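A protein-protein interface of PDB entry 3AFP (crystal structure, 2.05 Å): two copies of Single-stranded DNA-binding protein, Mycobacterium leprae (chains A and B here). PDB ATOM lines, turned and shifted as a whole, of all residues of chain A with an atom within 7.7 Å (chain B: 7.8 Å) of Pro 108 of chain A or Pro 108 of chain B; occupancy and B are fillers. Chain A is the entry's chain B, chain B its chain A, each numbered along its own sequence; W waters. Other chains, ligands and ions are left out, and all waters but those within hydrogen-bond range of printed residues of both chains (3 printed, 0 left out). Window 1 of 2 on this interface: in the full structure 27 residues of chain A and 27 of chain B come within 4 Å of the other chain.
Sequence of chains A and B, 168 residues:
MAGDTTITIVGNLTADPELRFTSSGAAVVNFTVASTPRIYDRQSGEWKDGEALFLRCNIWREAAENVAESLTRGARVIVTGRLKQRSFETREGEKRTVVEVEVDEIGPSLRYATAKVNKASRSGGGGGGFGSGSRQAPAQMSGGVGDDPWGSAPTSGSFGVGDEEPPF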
ATOM      1  N   SER A  70      -3.597  29.791   4.582  1.00  0.00           N
ATOM      2  CA  SER A  70      -3.134  28.415   4.488  1.00  0.00           C
ATOM      3  C   SER A  70      -3.290  27.739   3.126  1.00  0.00           C
ATOM      4  O   SER A  70      -2.461  26.917   2.788  1.00  0.00           O
ATOM      5  CB  SER A  70      -3.837  27.550   5.558  1.00  0.00           C
ATOM      6  OG  SER A  70      -3.800  28.169   6.831  1.00  0.00           O
ATOM      7  N   LEU A  71      -4.330  28.046   2.356  1.00  0.00           N
ATOM      8  CA  LEU A  71      -4.619  27.240   1.174  1.00  0.00           C
ATOM      9  C   LEU A  71      -4.347  27.970  -0.154  1.00  0.00           C
ATOM     10  O   LEU A  71      -4.505  29.189  -0.260  1.00  0.00           O
ATOM     11  CB  LEU A  71      -6.072  26.728   1.197  1.00  0.00           C
ATOM     12  CG  LEU A  71      -6.477  25.986   2.492  1.00  0.00           C
ATOM     13  CD1 LEU A  71      -7.926  25.534   2.400  1.00  0.00           C
ATOM     14  CD2 LEU A  71      -5.527  24.818   2.799  1.00  0.00           C
ATOM     15  N   ALA A  75      -5.210  22.943  -3.967  1.00  0.00           N
ATOM     16  CA  ALA A  75      -5.099  22.233  -2.687  1.00  0.00           C
ATOM     17  C   ALA A  75      -6.276  21.261  -2.539  1.00  0.00           C
ATOM     18  O   ALA A  75      -7.404  21.598  -2.850  1.00  0.00           O
ATOM     19  CB  ALA A  75      -5.031  23.205  -1.506  1.00  0.00           C
ATOM     20  N   ARG A  76      -5.973  20.050  -2.121  1.00  0.00           N
ATOM     21  CA  ARG A  76      -6.981  19.044  -1.770  1.00  0.00           C
ATOM     22  C   ARG A  76      -7.509  19.364  -0.415  1.00  0.00           C
ATOM     23  O   ARG A  76      -6.734  19.409   0.540  1.00  0.00           O
ATOM     24  CB  ARG A  76      -6.342  17.652  -1.692  1.00  0.00           C
ATOM     25  CG  ARG A  76      -7.411  16.531  -1.739  1.00  0.00           C
ATOM     26  CD  ARG A  76      -6.776  15.128  -1.739  1.00  0.00           C
ATOM     27  NE  ARG A  76      -7.763  14.035  -1.667  1.00  0.00           N
ATOM     28  CZ  ARG A  76      -8.479  13.615  -2.701  1.00  0.00           C
ATOM     29  NH1 ARG A  76      -8.333  14.196  -3.903  1.00  0.00           N
ATOM     30  NH2 ARG A  76      -9.360  12.613  -2.551  1.00  0.00           N
ATOM     31  N   VAL A  77      -8.826  19.504  -0.303  1.00  0.00           N
ATOM     32  CA  VAL A  77      -9.472  19.870   0.932  1.00  0.00           C
ATOM     33  C   VAL A  77     -10.695  19.000   1.295  1.00  0.00           C
ATOM     34  O   VAL A  77     -11.352  18.391   0.438  1.00  0.00           O
ATOM     35  CB  VAL A  77      -9.940  21.357   0.861  1.00  0.00           C
ATOM     36  CG1 VAL A  77      -8.769  22.303   0.681  1.00  0.00           C
ATOM     37  CG2 VAL A  77     -10.961  21.551  -0.284  1.00  0.00           C
ATOM     38  N   ILE A  78     -11.010  18.982   2.579  1.00  0.00           N
ATOM     39  CA  ILE A  78     -12.167  18.325   3.105  1.00  0.00           C
ATOM     40  C   ILE A  78     -13.003  19.461   3.684  1.00  0.00           C
ATOM     41  O   ILE A  78     -12.513  20.249   4.488  1.00  0.00           O
ATOM     42  CB  ILE A  78     -11.819  17.427   4.279  1.00  0.00           C
ATOM     43  CG1 ILE A  78     -10.688  16.486   3.915  1.00  0.00           C
ATOM     44  CG2 ILE A  78     -13.094  16.702   4.767  1.00  0.00           C
ATOM     45  CD1 ILE A  78     -10.333  15.544   5.120  1.00  0.00           C
ATOM     46  N   VAL A  79     -14.254  19.530   3.273  1.00  0.00           N
ATOM     47  CA  VAL A  79     -15.098  20.634   3.646  1.00  0.00           C
ATOM     48  C   VAL A  79     -16.366  20.092   4.175  1.00  0.00           C
ATOM     49  O   VAL A  79     -16.998  19.243   3.519  1.00  0.00           O
ATOM     50  CB  VAL A  79     -15.436  21.530   2.433  1.00  0.00           C
ATOM     51  CG1 VAL A  79     -16.403  22.620   2.810  1.00  0.00           C
ATOM     52  CG2 VAL A  79     -14.122  22.070   1.729  1.00  0.00           C
ATOM     53  N   GLU A 105     -16.553  23.589   8.585  1.00  0.00           N
ATOM     54  CA  GLU A 105     -15.112  23.255   8.827  1.00  0.00           C
ATOM     55  C   GLU A 105     -14.472  22.954   7.497  1.00  0.00           C
ATOM     56  O   GLU A 105     -15.119  22.382   6.603  1.00  0.00           O
ATOM     57  CB  GLU A 105     -14.996  21.994   9.724  1.00  0.00           C
ATOM     58  CG  GLU A 105     -15.897  22.092  10.975  1.00  0.00           C
ATOM     59  CD  GLU A 105     -15.124  22.501  12.221  1.00  0.00           C
ATOM     60  OE1 GLU A 105     -13.855  22.574  12.223  1.00  0.00           O
ATOM     61  OE2 GLU A 105     -15.776  22.656  13.228  1.00  0.00           O
ATOM     62  N   ILE A 106     -13.202  23.326   7.377  1.00  0.00           N
ATOM     63  CA  ILE A 106     -12.429  23.047   6.188  1.00  0.00           C
ATOM     64  C   ILE A 106     -10.995  22.803   6.613  1.00  0.00           C
ATOM     65  O   ILE A 106     -10.473  23.454   7.526  1.00  0.00           O
ATOM     66  CB  ILE A 106     -12.444  24.200   5.116  1.00  0.00           C
ATOM     67  CG1 ILE A 106     -11.473  23.860   3.995  1.00  0.00           C
ATOM     68  CG2 ILE A 106     -11.995  25.563   5.725  1.00  0.00           C
ATOM     69  CD1 ILE A 106     -11.743  24.681   2.710  1.00  0.00           C
ATOM     70  N   GLY A 107     -10.368  21.855   5.930  1.00  0.00           N
ATOM     71  CA  GLY A 107      -9.001  21.493   6.202  1.00  0.00           C
ATOM     72  C   GLY A 107      -8.300  20.938   4.984  1.00  0.00           C
ATOM     73  O   GLY A 107      -8.961  20.348   4.106  1.00  0.00           O
ATOM     74  N   PRO A 108      -6.976  21.138   4.883  1.00  0.00           N
ATOM     75  CA  PRO A 108      -6.267  20.441   3.798  1.00  0.00           C
ATOM     76  C   PRO A 108      -6.230  18.897   4.044  1.00  0.00           C
ATOM     77  O   PRO A 108      -5.873  18.418   5.126  1.00  0.00           O
ATOM     78  CB  PRO A 108      -4.816  20.982   3.919  1.00  0.00           C
ATOM     79  CG  PRO A 108      -4.670  21.230   5.410  1.00  0.00           C
ATOM     80  CD  PRO A 108      -6.043  21.864   5.768  1.00  0.00           C
ATOM     81  N   SER A 109      -6.542  18.141   3.019  1.00  0.00           N
ATOM     82  CA  SER A 109      -6.481  16.688   3.154  1.00  0.00           C
ATOM     83  C   SER A 109      -5.028  16.235   3.228  1.00  0.00           C
ATOM     84  O   SER A 109      -4.168  16.781   2.528  1.00  0.00           O
ATOM     85  CB  SER A 109      -7.176  16.010   1.956  1.00  0.00           C
ATOM     86  OG  SER A 109      -6.834  14.637   1.985  1.00  0.00           O
ATOM     87  N   LEU A 110      -4.767  15.228   4.055  1.00  0.00           N
ATOM     88  CA  LEU A 110      -3.440  14.654   4.198  1.00  0.00           C
ATOM     89  C   LEU A 110      -3.257  13.401   3.316  1.00  0.00           C
ATOM     90  O   LEU A 110      -2.355  12.638   3.538  1.00  0.00           O
ATOM     91  CB  LEU A 110      -3.176  14.268   5.666  1.00  0.00           C
ATOM     92  CG  LEU A 110      -3.345  15.472   6.605  1.00  0.00           C
ATOM     93  CD1 LEU A 110      -3.133  15.051   8.005  1.00  0.00           C
ATOM     94  CD2 LEU A 110      -2.381  16.608   6.167  1.00  0.00           C
ATOM     95  N   ARG A 111      -4.120  13.221   2.318  1.00  0.00           N
ATOM     96  CA  ARG A 111      -4.041  12.059   1.487  1.00  0.00           C
ATOM     97  C   ARG A 111      -2.716  12.097   0.679  1.00  0.00           C
ATOM     98  O   ARG A 111      -1.949  11.117   0.702  1.00  0.00           O
ATOM     99  CB  ARG A 111      -5.254  11.962   0.601  1.00  0.00           C
ATOM    100  CG  ARG A 111      -5.164  10.807  -0.405  1.00  0.00           C
ATOM    101  CD  ARG A 111      -6.272  10.923  -1.423  1.00  0.00           C
ATOM    102  NE  ARG A 111      -7.551  10.416  -0.941  1.00  0.00           N
ATOM    103  CZ  ARG A 111      -7.863   9.130  -0.850  1.00  0.00           C
ATOM    104  NH1 ARG A 111      -9.069   8.787  -0.420  1.00  0.00           N
ATOM    105  NH2 ARG A 111      -6.965   8.193  -1.176  1.00  0.00           N
ATOM    106  N   ALA A 113      -0.440  14.927   0.987  1.00  0.00           N
ATOM    107  CA  ALA A 113       0.297  16.072   1.483  1.00  0.00           C
ATOM    108  C   ALA A 113       0.451  15.979   2.958  1.00  0.00           C
ATOM    109  O   ALA A 113      -0.297  15.260   3.626  1.00  0.00           O
ATOM    110  CB  ALA A 113      -0.419  17.350   1.122  1.00  0.00           C
ATOM    111  N   THR A 114       1.474  16.662   3.463  1.00  0.00           N
ATOM    112  CA  THR A 114       1.687  16.802   4.906  1.00  0.00           C
ATOM    113  C   THR A 114       1.321  18.246   5.256  1.00  0.00           C
ATOM    114  O   THR A 114       1.109  19.082   4.367  1.00  0.00           O
ATOM    115  CB  THR A 114       3.155  16.571   5.325  1.00  0.00           C
ATOM    116  OG1 THR A 114       3.981  17.559   4.683  1.00  0.00           O
ATOM    117  CG2 THR A 114       3.626  15.167   4.959  1.00  0.00           C
ATOM    118  N   ALA A 115       1.215  18.532   6.549  1.00  0.00           N
ATOM    119  CA  ALA A 115       0.870  19.885   6.972  1.00  0.00           C
ATOM    120  C   ALA A 115       1.519  20.188   8.279  1.00  0.00           C
ATOM    121  O   ALA A 115       1.705  19.295   9.110  1.00  0.00           O
ATOM    122  CB  ALA A 115      -0.635  20.068   7.074  1.00  0.00           C
ATOM    123  N   LYS A 116       1.900  21.444   8.455  1.00  0.00           N
ATOM    124  CA  LYS A 116       2.386  21.909   9.745  1.00  0.00           C
ATOM    125  C   LYS A 116       1.301  22.869  10.259  1.00  0.00           C
ATOM    126  O   LYS A 116       1.074  23.944   9.675  1.00  0.00           O
ATOM    127  CB  LYS A 116       3.746  22.625   9.567  1.00  0.00           C
ATOM    128  CG  LYS A 116       4.317  23.226  10.847  1.00  0.00           C
ATOM    129  CD  LYS A 116       5.517  24.096  10.546  1.00  0.00           C
ATOM    130  CE  LYS A 116       5.963  24.802  11.783  1.00  0.00           C
ATOM    131  NZ  LYS A 116       7.231  25.544  11.525  1.00  0.00           N
ATOM    132  N   VAL A 117       0.614  22.445  11.304  1.00  0.00           N
ATOM    133  CA  VAL A 117      -0.486  23.161  11.892  1.00  0.00           C
ATOM    134  C   VAL A 117      -0.016  24.120  12.997  1.00  0.00           C
ATOM    135  O   VAL A 117       0.741  23.756  13.902  1.00  0.00           O
ATOM    136  CB  VAL A 117      -1.523  22.173  12.505  1.00  0.00           C
ATOM    137  CG1 VAL A 117      -2.709  22.919  13.099  1.00  0.00           C
ATOM    138  CG2 VAL A 117      -1.998  21.190  11.439  1.00  0.00           C
ATOM    139  N   ASN A 118      -0.538  25.326  12.955  1.00  0.00           N
ATOM    140  CA  ASN A 118      -0.256  26.307  13.976  1.00  0.00           C
ATOM    141  C   ASN A 118      -1.579  26.794  14.594  1.00  0.00           C
ATOM    142  O   ASN A 118      -2.381  27.432  13.917  1.00  0.00           O
ATOM    143  CB  ASN A 118       0.597  27.431  13.354  1.00  0.00           C
ATOM    144  CG  ASN A 118       1.903  26.889  12.687  1.00  0.00           C
ATOM    145  OD1 ASN A 118       2.847  26.450  13.382  1.00  0.00           O
ATOM    146  ND2 ASN A 118       1.948  26.899  11.334  1.00  0.00           N
ATOM    147  N   GLY B  11     -13.309  16.534  15.492  1.00  0.00           N
ATOM    148  CA  GLY B  11     -12.964  16.551  16.903  1.00  0.00           C
ATOM    149  C   GLY B  11     -11.486  16.652  17.083  1.00  0.00           C
ATOM    150  O   GLY B  11     -10.793  17.033  16.160  1.00  0.00           O
ATOM    151  N   SER B  70       2.272  14.918  10.400  1.00  0.00           N
ATOM    152  CA  SER B  70       1.611  16.235  10.458  1.00  0.00           C
ATOM    153  C   SER B  70       0.927  16.528  11.782  1.00  0.00           C
ATOM    154  O   SER B  70       0.920  17.677  12.208  1.00  0.00           O
ATOM    155  CB  SER B  70       0.577  16.397   9.339  1.00  0.00           C
ATOM    156  OG  SER B  70       1.130  16.044   8.098  1.00  0.00           O
ATOM    157  N   LEU B  71       0.324  15.520  12.420  1.00  0.00           N
ATOM    158  CA  LEU B  71      -0.627  15.775  13.497  1.00  0.00           C
ATOM    159  C   LEU B  71      -0.106  15.391  14.859  1.00  0.00           C
ATOM    160  O   LEU B  71       0.735  14.509  14.987  1.00  0.00           O
ATOM    161  CB  LEU B  71      -1.974  15.030  13.236  1.00  0.00           C
ATOM    162  CG  LEU B  71      -2.722  15.442  11.972  1.00  0.00           C
ATOM    163  CD1 LEU B  71      -4.038  14.708  11.811  1.00  0.00           C
ATOM    164  CD2 LEU B  71      -2.900  16.982  11.952  1.00  0.00           C
ATOM    165  N   ALA B  75      -4.913  18.000  18.164  1.00  0.00           N
ATOM    166  CA  ALA B  75      -5.191  18.626  16.873  1.00  0.00           C
ATOM    167  C   ALA B  75      -6.669  18.443  16.499  1.00  0.00           C
ATOM    168  O   ALA B  75      -7.221  17.329  16.596  1.00  0.00           O
ATOM    169  CB  ALA B  75      -4.325  18.029  15.748  1.00  0.00           C
ATOM    170  N   ARG B  76      -7.279  19.525  16.013  1.00  0.00           N
ATOM    171  CA  ARG B  76      -8.659  19.486  15.615  1.00  0.00           C
ATOM    172  C   ARG B  76      -8.649  18.949  14.190  1.00  0.00           C
ATOM    173  O   ARG B  76      -7.934  19.495  13.312  1.00  0.00           O
ATOM    174  CB  ARG B  76      -9.269  20.910  15.620  1.00  0.00           C
ATOM    175  CG  ARG B  76     -10.776  20.899  15.201  1.00  0.00           C
ATOM    176  CD  ARG B  76     -11.349  22.299  15.233  1.00  0.00           C
ATOM    177  NE  ARG B  76     -12.776  22.336  15.018  1.00  0.00           N
ATOM    178  CZ  ARG B  76     -13.667  22.201  16.007  1.00  0.00           C
ATOM    179  NH1 ARG B  76     -14.964  22.300  15.747  1.00  0.00           N
ATOM    180  NH2 ARG B  76     -13.241  22.018  17.242  1.00  0.00           N
ATOM    181  N   VAL B  77      -9.434  17.895  13.944  1.00  0.00           N
ATOM    182  CA  VAL B  77      -9.407  17.225  12.658  1.00  0.00           C
ATOM    183  C   VAL B  77     -10.795  17.041  12.118  1.00  0.00           C
ATOM    184  O   VAL B  77     -11.778  16.995  12.862  1.00  0.00           O
ATOM    185  CB  VAL B  77      -8.670  15.847  12.720  1.00  0.00           C
ATOM    186  CG1 VAL B  77      -7.171  16.050  13.120  1.00  0.00           C
ATOM    187  CG2 VAL B  77      -9.361  14.895  13.747  1.00  0.00           C
ATOM    188  N   ILE B  78     -10.870  16.937  10.803  1.00  0.00           N
ATOM    189  CA  ILE B  78     -12.115  16.633  10.125  1.00  0.00           C
ATOM    190  C   ILE B  78     -11.849  15.241   9.525  1.00  0.00           C
ATOM    191  O   ILE B  78     -10.865  15.068   8.832  1.00  0.00           O
ATOM    192  CB  ILE B  78     -12.394  17.586   8.979  1.00  0.00           C
ATOM    193  CG1 ILE B  78     -12.426  19.025   9.488  1.00  0.00           C
ATOM    194  CG2 ILE B  78     -13.786  17.253   8.371  1.00  0.00           C
ATOM    195  CD1 ILE B  78     -12.126  19.995   8.370  1.00  0.00           C
ATOM    196  N   VAL B  79     -12.697  14.274   9.860  1.00  0.00           N
ATOM    197  CA  VAL B  79     -12.465  12.901   9.417  1.00  0.00           C
ATOM    198  C   VAL B  79     -13.702  12.370   8.743  1.00  0.00           C
ATOM    199  O   VAL B  79     -14.798  12.512   9.254  1.00  0.00           O
ATOM    200  CB  VAL B  79     -12.115  11.985  10.576  1.00  0.00           C
ATOM    201  CG1 VAL B  79     -12.113  10.531  10.133  1.00  0.00           C
ATOM    202  CG2 VAL B  79     -10.734  12.364  11.173  1.00  0.00           C
ATOM    203  N   GLU B 105     -10.746  10.145   4.257  1.00  0.00           N
ATOM    204  CA  GLU B 105      -9.983  11.393   4.202  1.00  0.00           C
ATOM    205  C   GLU B 105      -9.874  12.000   5.601  1.00  0.00           C
ATOM    206  O   GLU B 105     -10.786  11.859   6.426  1.00  0.00           O
ATOM    207  CB  GLU B 105     -10.670  12.422   3.279  1.00  0.00           C
ATOM    208  CG  GLU B 105     -10.917  11.983   1.874  1.00  0.00           C
ATOM    209  CD  GLU B 105      -9.770  12.203   0.876  1.00  0.00           C
ATOM    210  OE1 GLU B 105      -8.774  12.934   1.094  1.00  0.00           O
ATOM    211  OE2 GLU B 105      -9.928  11.658  -0.202  1.00  0.00           O
ATOM    212  N   ILE B 106      -8.746  12.636   5.883  1.00  0.00           N
ATOM    213  CA  ILE B 106      -8.563  13.335   7.146  1.00  0.00           C
ATOM    214  C   ILE B 106      -7.685  14.590   6.879  1.00  0.00           C
ATOM    215  O   ILE B 106      -6.783  14.556   6.056  1.00  0.00           O
ATOM    216  CB  ILE B 106      -7.885  12.485   8.229  1.00  0.00           C
ATOM    217  CG1 ILE B 106      -7.502  13.354   9.417  1.00  0.00           C
ATOM    218  CG2 ILE B 106      -6.521  11.825   7.686  1.00  0.00           C
ATOM    219  CD1 ILE B 106      -7.243  12.553  10.689  1.00  0.00           C
ATOM    220  N   GLY B 107      -8.011  15.688   7.566  1.00  0.00           N
ATOM    221  CA  GLY B 107      -7.194  16.907   7.537  1.00  0.00           C
ATOM    222  C   GLY B 107      -7.391  17.696   8.817  1.00  0.00           C
ATOM    223  O   GLY B 107      -8.472  17.620   9.453  1.00  0.00           O
ATOM    224  N   PRO B 108      -6.377  18.491   9.180  1.00  0.00           N
ATOM    225  CA  PRO B 108      -6.533  19.371  10.317  1.00  0.00           C
ATOM    226  C   PRO B 108      -7.491  20.503   9.973  1.00  0.00           C
ATOM    227  O   PRO B 108      -7.418  21.104   8.875  1.00  0.00           O
ATOM    228  CB  PRO B 108      -5.074  19.869  10.585  1.00  0.00           C
ATOM    229  CG  PRO B 108      -4.437  19.844   9.216  1.00  0.00           C
ATOM    230  CD  PRO B 108      -5.100  18.720   8.448  1.00  0.00           C
ATOM    231  N   SER B 109      -8.442  20.754  10.836  1.00  0.00           N
ATOM    232  CA  SER B 109      -9.380  21.892  10.583  1.00  0.00           C
ATOM    233  C   SER B 109      -8.666  23.251  10.689  1.00  0.00           C
ATOM    234  O   SER B 109      -7.836  23.459  11.575  1.00  0.00           O
ATOM    235  CB  SER B 109     -10.518  21.923  11.604  1.00  0.00           C
ATOM    236  OG  SER B 109     -11.396  23.001  11.299  1.00  0.00           O
ATOM    237  N   LEU B 110      -9.066  24.180   9.844  1.00  0.00           N
ATOM    238  CA  LEU B 110      -8.512  25.538   9.860  1.00  0.00           C
ATOM    239  C   LEU B 110      -9.479  26.453  10.593  1.00  0.00           C
ATOM    240  O   LEU B 110      -9.395  27.682  10.475  1.00  0.00           O
ATOM    241  CB  LEU B 110      -8.350  26.040   8.406  1.00  0.00           C
ATOM    242  CG  LEU B 110      -7.412  25.190   7.578  1.00  0.00           C
ATOM    243  CD1 LEU B 110      -7.274  25.720   6.116  1.00  0.00           C
ATOM    244  CD2 LEU B 110      -6.063  25.100   8.243  1.00  0.00           C
ATOM    245  N   ARG B 111     -10.412  25.873  11.340  1.00  0.00           N
ATOM    246  CA  ARG B 111     -11.355  26.692  12.079  1.00  0.00           C
ATOM    247  C   ARG B 111     -10.658  27.592  13.129  1.00  0.00           C
ATOM    248  O   ARG B 111     -11.012  28.758  13.296  1.00  0.00           O
ATOM    249  CB  ARG B 111     -12.387  25.824  12.818  1.00  0.00           C
ATOM    250  CG  ARG B 111     -13.385  26.709  13.541  1.00  0.00           C
ATOM    251  CD  ARG B 111     -14.223  25.980  14.502  1.00  0.00           C
ATOM    252  NE  ARG B 111     -15.386  25.401  13.880  1.00  0.00           N
ATOM    253  CZ  ARG B 111     -16.632  25.857  13.993  1.00  0.00           C
ATOM    254  NH1 ARG B 111     -16.901  26.954  14.705  1.00  0.00           N
ATOM    255  NH2 ARG B 111     -17.620  25.181  13.389  1.00  0.00           N
ATOM    256  N   ALA B 113      -7.114  27.466  13.387  1.00  0.00           N
ATOM    257  CA  ALA B 113      -5.685  27.350  13.134  1.00  0.00           C
ATOM    258  C   ALA B 113      -5.341  27.638  11.703  1.00  0.00           C
ATOM    259  O   ALA B 113      -6.201  27.636  10.842  1.00  0.00           O
ATOM    260  CB  ALA B 113      -5.163  25.923  13.531  1.00  0.00           C
ATOM    261  N   THR B 114      -4.059  27.884  11.439  1.00  0.00           N
ATOM    262  CA  THR B 114      -3.585  27.967  10.054  1.00  0.00           C
ATOM    263  C   THR B 114      -2.689  26.752   9.855  1.00  0.00           C
ATOM    264  O   THR B 114      -2.313  26.120  10.837  1.00  0.00           O
ATOM    265  CB  THR B 114      -2.717  29.237   9.861  1.00  0.00           C
ATOM    266  OG1 THR B 114      -1.654  29.187  10.823  1.00  0.00           O
ATOM    267  CG2 THR B 114      -3.548  30.476  10.125  1.00  0.00           C
ATOM    268  N   ALA B 115      -2.265  26.475   8.624  1.00  0.00           N
ATOM    269  CA  ALA B 115      -1.342  25.376   8.425  1.00  0.00           C
ATOM    270  C   ALA B 115      -0.441  25.613   7.228  1.00  0.00           C
ATOM    271  O   ALA B 115      -0.855  26.211   6.217  1.00  0.00           O
ATOM    272  CB  ALA B 115      -2.120  24.032   8.263  1.00  0.00           C
ATOM    273  N   LYS B 116       0.794  25.130   7.341  1.00  0.00           N
ATOM    274  CA  LYS B 116       1.692  25.143   6.186  1.00  0.00           C
ATOM    275  C   LYS B 116       1.504  23.804   5.463  1.00  0.00           C
ATOM    276  O   LYS B 116       1.798  22.761   6.029  1.00  0.00           O
ATOM    277  CB  LYS B 116       3.152  25.309   6.635  1.00  0.00           C
ATOM    278  CG  LYS B 116       4.040  26.018   5.632  1.00  0.00           C
ATOM    279  CD  LYS B 116       4.129  25.290   4.311  1.00  0.00           C
ATOM    280  CE  LYS B 116       5.051  26.017   3.319  1.00  0.00           C
ATOM    281  NZ  LYS B 116       6.500  25.806   3.650  1.00  0.00           N
ATOM    282  N   VAL B 117       1.004  23.854   4.231  1.00  0.00           N
ATOM    283  CA  VAL B 117       0.719  22.651   3.472  1.00  0.00           C
ATOM    284  C   VAL B 117       1.801  22.374   2.422  1.00  0.00           C
ATOM    285  O   VAL B 117       2.039  23.196   1.542  1.00  0.00           O
ATOM    286  CB  VAL B 117      -0.674  22.736   2.797  1.00  0.00           C
ATOM    287  CG1 VAL B 117      -0.944  21.499   1.928  1.00  0.00           C
ATOM    288  CG2 VAL B 117      -1.758  22.915   3.851  1.00  0.00           C
ATOM    289  N   ASN B 118       2.398  21.184   2.500  1.00  0.00           N
ATOM    290  CA  ASN B 118       3.421  20.762   1.578  1.00  0.00           C
ATOM    291  C   ASN B 118       3.039  19.446   0.890  1.00  0.00           C
ATOM    292  O   ASN B 118       2.917  18.410   1.542  1.00  0.00           O
ATOM    293  CB  ASN B 118       4.736  20.613   2.338  1.00  0.00           C
ATOM    294  CG  ASN B 118       5.275  21.956   2.884  1.00  0.00           C
ATOM    295  OD1 ASN B 118       5.462  22.935   2.138  1.00  0.00           O
ATOM    296  ND2 ASN B 118       5.549  21.992   4.191  1.00  0.00           N
HETATM  297  O   HOH W   1       1.580  20.221  12.667  1.00  0.00           O
HETATM  298  O   HOH W   2      -6.588  12.153   3.834  1.00  0.00           O
HETATM  299  O   HOH W   3     -12.582  25.483   9.299  1.00  0.00           O
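N of Ala 115 of chain A sits at hydrogen-bond distance from OG of Ser 70 of chain B, 2.9 Å away. NH1 of Arg 76 of chain B is in salt-bridge range of OE2 of Glu 105 of chain A, 2.7 Å away. The side-chain carboxylate of Glu 105 of chain B lies within salt-bridge range of the guanidinium group of Arg 76 of chain A (2.6 Å). The side-chain hydroxyl of Ser 109 of chain A sits at hydrogen-bond distance from the side-chain carboxylate of Glu 105 of chain B (2.7 Å). The guanidinium group (NE) of Arg 111 of chain A is in salt-bridge range of the side-chain carboxylate (OE2) of Glu 105 of chain B (2.8 Å). O of Ile 106 of chain B sits at hydrogen-bond distance from N of Leu 110 of chain A (2.9 Å). OE1 of Glu 105 of chain A is in hydrogen-bond range of OG of Ser 109 of chain B (2.7 Å). N of Leu 110 of chain B lies within hydrogen-bond range of O of Ile 106 of chain A, at 2.8 Å. NE of Arg 111 of chain B is in salt-bridge range of OE2 of Glu 105 of chain A. O of Thr 114 of chain B lies within hydrogen-bond range of N of Asn 118 of chain A (2.9 Å). N of Ala 115 of chain B lies within hydrogen-bond range of OG of Ser 70 of chain A, at 2.9 Å. The backbone NH of Lys 116 of chain B lies within hydrogen-bond range of the backbone carbonyl oxygen of Lys 116 of chain A. The backbone NH of Thr 114 of chain A sits at hydrogen-bond distance from the backbone carbonyl oxygen of Asn 118 of chain B (3.0 Å).
N of Ile 78 of chain B lies within hydrogen-bond range of O of Gly 107 of chain B, 2.8 Å away. The side-chain amide oxygen (OD1) of Asn 118 of chain B sits close to the side-chain amino group (NZ) of Lys 116 of chain B, 3.4 Å away.
Gly 107 of chain A touches two residues of chain B. Of chain A, only Gly 107 (3.1 Å), Pro 108 (3.4 Å) and Val 117 (3.5 Å) come within 4 Å of Pro 108 of chain B. Of the printed residues of chain A, Ser 109 of chain B touches Glu 105 and Ile 106. Of the printed residues of chain A, Thr 114 of chain B touches Ser 70, Val 117 and Asn 118. The nearest residue of chain B that does not touch Pro 108 of chain A is Leu 110 of chain B (4.03 Å).
Hydrophobic or aromatic side chains of chain A that line the printed part of chain B: Leu 71, Ile 78, Pro 108, Leu 110, Ala 113, Ala 115 and Val 117. Among the printed residues, 39 pairs touch across the chains.
Ile 78 of chain A touches Glu 105 of chain B, and with the chains exchanged Glu 105 of chain A touches Ile 78 of chain B. Pro 108 of chain A touches its own counterpart, Pro 108 of chain B.
Water W1 bridges O of Ser 70 of chain B and N of Val 117 of chain A.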
